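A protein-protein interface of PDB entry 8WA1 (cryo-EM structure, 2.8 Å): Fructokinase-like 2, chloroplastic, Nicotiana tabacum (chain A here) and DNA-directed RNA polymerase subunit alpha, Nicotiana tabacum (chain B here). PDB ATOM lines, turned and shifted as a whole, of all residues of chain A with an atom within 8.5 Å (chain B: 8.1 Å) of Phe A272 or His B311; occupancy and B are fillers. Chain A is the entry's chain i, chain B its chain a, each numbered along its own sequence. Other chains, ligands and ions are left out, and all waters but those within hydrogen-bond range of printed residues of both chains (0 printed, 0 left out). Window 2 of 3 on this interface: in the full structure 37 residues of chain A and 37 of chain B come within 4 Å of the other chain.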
ATOM      1  N   GLU A 268       6.516  24.410 -19.099  1.00  0.00           N
ATOM      2  CA  GLU A 268       6.769  23.958 -20.462  1.00  0.00           C
ATOM      3  C   GLU A 268       5.551  23.265 -21.060  1.00  0.00           C
ATOM      4  O   GLU A 268       5.089  22.246 -20.548  1.00  0.00           O
ATOM      5  CB  GLU A 268       7.974  23.015 -20.499  1.00  0.00           C
ATOM      6  CG  GLU A 268       9.317  23.708 -20.333  1.00  0.00           C
ATOM      7  CD  GLU A 268       9.710  24.520 -21.554  1.00  0.00           C
ATOM      8  OE1 GLU A 268       9.148  24.272 -22.643  1.00  0.00           O
ATOM      9  OE2 GLU A 268      10.581  25.405 -21.425  1.00  0.00           O
ATOM     10  N   ASP A 269       5.033  23.827 -22.149  1.00  0.00           N
ATOM     11  CA  ASP A 269       3.912  23.249 -22.876  1.00  0.00           C
ATOM     12  C   ASP A 269       4.361  22.424 -24.075  1.00  0.00           C
ATOM     13  O   ASP A 269       3.558  22.183 -24.983  1.00  0.00           O
ATOM     14  CB  ASP A 269       2.949  24.348 -23.327  1.00  0.00           C
ATOM     15  CG  ASP A 269       3.617  25.384 -24.208  1.00  0.00           C
ATOM     16  OD1 ASP A 269       4.833  25.612 -24.041  1.00  0.00           O
ATOM     17  OD2 ASP A 269       2.925  25.970 -25.068  1.00  0.00           O
ATOM     18  N   ILE A 270       5.624  21.993 -24.102  1.00  0.00           N
ATOM     19  CA  ILE A 270       6.128  21.219 -25.234  1.00  0.00           C
ATOM     20  C   ILE A 270       5.413  19.874 -25.324  1.00  0.00           C
ATOM     21  O   ILE A 270       4.822  19.533 -26.355  1.00  0.00           O
ATOM     22  CB  ILE A 270       7.655  21.047 -25.133  1.00  0.00           C
ATOM     23  CG1 ILE A 270       8.127  19.911 -26.044  1.00  0.00           C
ATOM     24  CG2 ILE A 270       8.084  20.821 -23.687  1.00  0.00           C
ATOM     25  CD1 ILE A 270       9.619  19.669 -26.004  1.00  0.00           C
ATOM     26  N   SER A 271       5.449  19.095 -24.242  1.00  0.00           N
ATOM     27  CA  SER A 271       4.802  17.787 -24.257  1.00  0.00           C
ATOM     28  C   SER A 271       3.284  17.917 -24.209  1.00  0.00           C
ATOM     29  O   SER A 271       2.565  16.987 -24.589  1.00  0.00           O
ATOM     30  CB  SER A 271       5.310  16.936 -23.090  1.00  0.00           C
ATOM     31  OG  SER A 271       6.700  16.678 -23.219  1.00  0.00           O
ATOM     32  N   PHE A 272       2.779  19.057 -23.734  1.00  0.00           N
ATOM     33  CA  PHE A 272       1.338  19.206 -23.557  1.00  0.00           C
ATOM     34  C   PHE A 272       0.613  19.406 -24.882  1.00  0.00           C
ATOM     35  O   PHE A 272      -0.280  18.621 -25.222  1.00  0.00           O
ATOM     36  CB  PHE A 272       1.046  20.376 -22.617  1.00  0.00           C
ATOM     37  CG  PHE A 272       1.545  20.168 -21.216  1.00  0.00           C
ATOM     38  CD1 PHE A 272       1.689  18.891 -20.696  1.00  0.00           C
ATOM     39  CD2 PHE A 272       1.865  21.252 -20.416  1.00  0.00           C
ATOM     40  CE1 PHE A 272       2.147  18.701 -19.407  1.00  0.00           C
ATOM     41  CE2 PHE A 272       2.324  21.067 -19.126  1.00  0.00           C
ATOM     42  CZ  PHE A 272       2.464  19.791 -18.622  1.00  0.00           C
ATOM     43  N   SER A 273       1.122  20.354 -25.678  1.00  0.00           N
ATOM     44  CA  SER A 273       0.436  20.696 -26.915  1.00  0.00           C
ATOM     45  C   SER A 273       1.252  21.030 -28.153  1.00  0.00           C
ATOM     46  O   SER A 273       0.771  21.767 -29.001  1.00  0.00           O
ATOM     47  CB  SER A 273      -0.432  21.906 -26.618  1.00  0.00           C
ATOM     48  OG  SER A 273       0.348  22.953 -26.071  1.00  0.00           O
ATOM     49  N   TYR A 274       2.479  20.558 -28.283  1.00  0.00           N
ATOM     50  CA  TYR A 274       3.185  20.856 -29.529  1.00  0.00           C
ATOM     51  C   TYR A 274       2.651  20.214 -30.825  1.00  0.00           C
ATOM     52  O   TYR A 274       2.550  20.898 -31.834  1.00  0.00           O
ATOM     53  CB  TYR A 274       4.693  20.690 -29.386  1.00  0.00           C
ATOM     54  CG  TYR A 274       5.361  21.878 -28.742  1.00  0.00           C
ATOM     55  CD1 TYR A 274       4.611  22.876 -28.136  1.00  0.00           C
ATOM     56  CD2 TYR A 274       6.738  22.008 -28.743  1.00  0.00           C
ATOM     57  CE1 TYR A 274       5.214  23.964 -27.545  1.00  0.00           C
ATOM     58  CE2 TYR A 274       7.351  23.093 -28.152  1.00  0.00           C
ATOM     59  CZ  TYR A 274       6.583  24.066 -27.555  1.00  0.00           C
ATOM     60  OH  TYR A 274       7.187  25.149 -26.969  1.00  0.00           O
ATOM     61  N   GLY A 275       2.306  18.931 -30.826  1.00  0.00           N
ATOM     62  CA  GLY A 275       1.713  18.316 -32.014  1.00  0.00           C
ATOM     63  C   GLY A 275       2.712  17.744 -32.997  1.00  0.00           C
ATOM     64  O   GLY A 275       3.862  18.163 -32.992  1.00  0.00           O
ATOM     65  N   ARG B 282      -0.825  27.610 -24.415  1.00  0.00           N
ATOM     66  CA  ARG B 282      -1.441  26.327 -24.083  1.00  0.00           C
ATOM     67  C   ARG B 282      -2.889  26.263 -24.554  1.00  0.00           C
ATOM     68  O   ARG B 282      -3.276  25.329 -25.267  1.00  0.00           O
ATOM     69  CB  ARG B 282      -1.366  26.085 -22.576  1.00  0.00           C
ATOM     70  CG  ARG B 282       0.044  26.037 -22.017  1.00  0.00           C
ATOM     71  CD  ARG B 282       0.024  25.757 -20.525  1.00  0.00           C
ATOM     72  NE  ARG B 282      -0.717  24.537 -20.213  1.00  0.00           N
ATOM     73  CZ  ARG B 282      -0.937  24.090 -18.981  1.00  0.00           C
ATOM     74  NH1 ARG B 282      -0.474  24.763 -17.936  1.00  0.00           N
ATOM     75  NH2 ARG B 282      -1.621  22.970 -18.792  1.00  0.00           N
ATOM     76  N   ILE B 283      -3.702  27.245 -24.161  1.00  0.00           N
ATOM     77  CA  ILE B 283      -5.117  27.229 -24.518  1.00  0.00           C
ATOM     78  C   ILE B 283      -5.286  27.366 -26.024  1.00  0.00           C
ATOM     79  O   ILE B 283      -6.147  26.716 -26.629  1.00  0.00           O
ATOM     80  CB  ILE B 283      -5.878  28.334 -23.760  1.00  0.00           C
ATOM     81  CG1 ILE B 283      -5.716  28.164 -22.248  1.00  0.00           C
ATOM     82  CG2 ILE B 283      -7.353  28.319 -24.134  1.00  0.00           C
ATOM     83  CD1 ILE B 283      -4.623  29.019 -21.639  1.00  0.00           C
ATOM     84  N   ASN B 285      -3.188  26.386 -28.467  1.00  0.00           N
ATOM     85  CA  ASN B 285      -2.853  25.134 -29.137  1.00  0.00           C
ATOM     86  C   ASN B 285      -3.885  24.052 -28.845  1.00  0.00           C
ATOM     87  O   ASN B 285      -4.209  23.243 -29.723  1.00  0.00           O
ATOM     88  CB  ASN B 285      -1.455  24.672 -28.726  1.00  0.00           C
ATOM     89  CG  ASN B 285      -0.363  25.581 -29.253  1.00  0.00           C
ATOM     90  OD1 ASN B 285       0.612  25.870 -28.559  1.00  0.00           O
ATOM     91  ND2 ASN B 285      -0.523  26.044 -30.488  1.00  0.00           N
ATOM     92  N   CYS B 286      -4.417  24.017 -27.618  1.00  0.00           N
ATOM     93  CA  CYS B 286      -5.431  23.018 -27.295  1.00  0.00           C
ATOM     94  C   CYS B 286      -6.715  23.256 -28.080  1.00  0.00           C
ATOM     95  O   CYS B 286      -7.362  22.301 -28.523  1.00  0.00           O
ATOM     96  CB  CYS B 286      -5.708  23.015 -25.793  1.00  0.00           C
ATOM     97  SG  CYS B 286      -4.357  22.360 -24.787  1.00  0.00           S
ATOM     98  N   MET B 289      -6.071  22.183 -31.677  1.00  0.00           N
ATOM     99  CA  MET B 289      -6.166  20.731 -31.795  1.00  0.00           C
ATOM    100  C   MET B 289      -7.611  20.258 -31.716  1.00  0.00           C
ATOM    101  O   MET B 289      -7.953  19.210 -32.275  1.00  0.00           O
ATOM    102  CB  MET B 289      -5.327  20.054 -30.711  1.00  0.00           C
ATOM    103  CG  MET B 289      -3.828  20.169 -30.918  1.00  0.00           C
ATOM    104  SD  MET B 289      -2.889  19.314 -29.637  1.00  0.00           S
ATOM    105  CE  MET B 289      -1.220  19.501 -30.259  1.00  0.00           C
ATOM    106  N   LEU B 306     -15.304  22.311 -23.189  1.00  0.00           N
ATOM    107  CA  LEU B 306     -13.961  22.856 -23.023  1.00  0.00           C
ATOM    108  C   LEU B 306     -13.176  22.071 -21.981  1.00  0.00           C
ATOM    109  O   LEU B 306     -11.986  21.794 -22.166  1.00  0.00           O
ATOM    110  CB  LEU B 306     -14.031  24.333 -22.635  1.00  0.00           C
ATOM    111  CG  LEU B 306     -14.473  25.323 -23.714  1.00  0.00           C
ATOM    112  CD1 LEU B 306     -14.523  26.734 -23.153  1.00  0.00           C
ATOM    113  CD2 LEU B 306     -13.546  25.255 -24.918  1.00  0.00           C
ATOM    114  N   MET B 307     -13.825  21.710 -20.872  1.00  0.00           N
ATOM    115  CA  MET B 307     -13.154  20.908 -19.854  1.00  0.00           C
ATOM    116  C   MET B 307     -12.905  19.488 -20.351  1.00  0.00           C
ATOM    117  O   MET B 307     -12.013  18.792 -19.850  1.00  0.00           O
ATOM    118  CB  MET B 307     -13.984  20.894 -18.570  1.00  0.00           C
ATOM    119  CG  MET B 307     -13.250  20.351 -17.355  1.00  0.00           C
ATOM    120  SD  MET B 307     -11.824  21.358 -16.906  1.00  0.00           S
ATOM    121  CE  MET B 307     -11.180  20.437 -15.511  1.00  0.00           C
ATOM    122  N   LYS B 308     -13.685  19.044 -21.340  1.00  0.00           N
ATOM    123  CA  LYS B 308     -13.577  17.670 -21.821  1.00  0.00           C
ATOM    124  C   LYS B 308     -12.232  17.410 -22.491  1.00  0.00           C
ATOM    125  O   LYS B 308     -11.704  16.295 -22.424  1.00  0.00           O
ATOM    126  CB  LYS B 308     -14.721  17.371 -22.790  1.00  0.00           C
ATOM    127  CG  LYS B 308     -15.173  15.922 -22.798  1.00  0.00           C
ATOM    128  CD  LYS B 308     -15.944  15.587 -21.533  1.00  0.00           C
ATOM    129  CE  LYS B 308     -17.184  16.459 -21.400  1.00  0.00           C
ATOM    130  NZ  LYS B 308     -17.941  16.170 -20.151  1.00  0.00           N
ATOM    131  N   ILE B 309     -11.665  18.426 -23.148  1.00  0.00           N
ATOM    132  CA  ILE B 309     -10.443  18.218 -23.915  1.00  0.00           C
ATOM    133  C   ILE B 309      -9.279  17.918 -22.979  1.00  0.00           C
ATOM    134  O   ILE B 309      -9.268  18.327 -21.810  1.00  0.00           O
ATOM    135  CB  ILE B 309     -10.145  19.440 -24.800  1.00  0.00           C
ATOM    136  CG1 ILE B 309      -9.689  20.626 -23.950  1.00  0.00           C
ATOM    137  CG2 ILE B 309     -11.369  19.810 -25.625  1.00  0.00           C
ATOM    138  CD1 ILE B 309      -9.384  21.869 -24.754  1.00  0.00           C
ATOM    139  N   GLU B 310      -8.293  17.190 -23.496  1.00  0.00           N
ATOM    140  CA  GLU B 310      -7.146  16.792 -22.696  1.00  0.00           C
ATOM    141  C   GLU B 310      -6.229  17.982 -22.428  1.00  0.00           C
ATOM    142  O   GLU B 310      -6.242  18.989 -23.142  1.00  0.00           O
ATOM    143  CB  GLU B 310      -6.366  15.679 -23.397  1.00  0.00           C
ATOM    144  N   HIS B 311      -5.420  17.846 -21.372  1.00  0.00           N
ATOM    145  CA  HIS B 311      -4.463  18.874 -20.960  1.00  0.00           C
ATOM    146  C   HIS B 311      -5.153  20.213 -20.708  1.00  0.00           C
ATOM    147  O   HIS B 311      -4.657  21.273 -21.096  1.00  0.00           O
ATOM    148  CB  HIS B 311      -3.336  19.027 -21.984  1.00  0.00           C
ATOM    149  CG  HIS B 311      -2.453  17.823 -22.099  1.00  0.00           C
ATOM    150  ND1 HIS B 311      -1.373  17.609 -21.269  1.00  0.00           N
ATOM    151  CD2 HIS B 311      -2.491  16.767 -22.947  1.00  0.00           C
ATOM    152  CE1 HIS B 311      -0.784  16.474 -21.601  1.00  0.00           C
ATOM    153  NE2 HIS B 311      -1.442  15.943 -22.616  1.00  0.00           N
ATOM    154  N   PHE B 312      -6.310  20.165 -20.052  1.00  0.00           N
ATOM    155  CA  PHE B 312      -7.073  21.358 -19.725  1.00  0.00           C
ATOM    156  C   PHE B 312      -7.468  21.323 -18.255  1.00  0.00           C
ATOM    157  O   PHE B 312      -7.609  20.255 -17.652  1.00  0.00           O
ATOM    158  CB  PHE B 312      -8.321  21.485 -20.608  1.00  0.00           C
ATOM    159  CG  PHE B 312      -8.356  22.739 -21.432  1.00  0.00           C
ATOM    160  CD1 PHE B 312      -7.260  23.117 -22.189  1.00  0.00           C
ATOM    161  CD2 PHE B 312      -9.490  23.532 -21.462  1.00  0.00           C
ATOM    162  CE1 PHE B 312      -7.292  24.270 -22.951  1.00  0.00           C
ATOM    163  CE2 PHE B 312      -9.528  24.683 -22.225  1.00  0.00           C
ATOM    164  CZ  PHE B 312      -8.427  25.053 -22.970  1.00  0.00           C
ATOM    165  N   ARG B 313      -7.644  22.510 -17.679  1.00  0.00           N
ATOM    166  CA  ARG B 313      -8.007  22.643 -16.277  1.00  0.00           C
ATOM    167  C   ARG B 313      -9.059  23.733 -16.130  1.00  0.00           C
ATOM    168  O   ARG B 313      -9.355  24.473 -17.070  1.00  0.00           O
ATOM    169  CB  ARG B 313      -6.786  22.959 -15.397  1.00  0.00           C
ATOM    170  CG  ARG B 313      -6.080  24.267 -15.726  1.00  0.00           C
ATOM    171  CD  ARG B 313      -4.986  24.075 -16.767  1.00  0.00           C
ATOM    172  NE  ARG B 313      -3.906  23.223 -16.278  1.00  0.00           N
ATOM    173  CZ  ARG B 313      -2.816  23.676 -15.669  1.00  0.00           C
ATOM    174  NH1 ARG B 313      -2.655  24.977 -15.471  1.00  0.00           N
ATOM    175  NH2 ARG B 313      -1.883  22.828 -15.256  1.00  0.00           N
ATOM    176  N   ASP B 316      -7.898  27.723 -16.734  1.00  0.00           N
ATOM    177  CA  ASP B 316      -7.907  28.377 -18.039  1.00  0.00           C
ATOM    178  C   ASP B 316      -9.315  28.767 -18.470  1.00  0.00           C
ATOM    179  O   ASP B 316      -9.481  29.678 -19.291  1.00  0.00           O
ATOM    180  CB  ASP B 316      -7.262  27.470 -19.087  1.00  0.00           C
ATOM    181  CG  ASP B 316      -7.901  26.095 -19.144  1.00  0.00           C
ATOM    182  OD1 ASP B 316      -9.098  26.005 -19.484  1.00  0.00           O
ATOM    183  OD2 ASP B 316      -7.203  25.103 -18.852  1.00  0.00           O
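The backbone carbonyl oxygen (O) of Arg B282 sits at hydrogen-bond distance from the side-chain sulfur (SG) of Cys B286 (3.2 Å).
The backbone carbonyl oxygen (O) of Asp A269 sits at hydrogen-bond distance from the side-chain hydroxyl (OG) of Ser A273, at 3.5 Å.
Among the printed residues, merely in contact across the chains: Asp A269 with Arg B282, Phe A272 with His B311, Ser A273 with Asn B285, Ser A273 with Met B289, Tyr A274 with Met B289 and Gly A275 with Met B289.
Of the printed residues of chain B, Tyr A274 touches Met B289.
Printed residues of chain A within 4 Å of Asn B285: Ser A273.
Of the printed residues of chain A, Met B289 touches Ser A273 (3.3 Å), Tyr A274 (3.98 Å) and Gly A275 (3.6 Å).
No residue of chain A comes within 4 Å of Glu B310.
Of chain A, only Phe A272 comes within 4 Å of His B311.
The nearest residue of chain B that does not touch Phe A272 is Arg B282 (4.2 Å).
Hydrophobic or aromatic side chains of chain B within 4 Å of the printed part of chain A: Met B289 and His B311.
Hydrophobic or aromatic side chains of chain A within 4 Å of the printed part of chain B: Phe A272.
Among the printed residues, 6 pairs touch across the chains.
Among the printed residues, no Asp or Glu carboxylate lies within 4 Å of a Lys or Arg side-chain nitrogen of the other chain.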
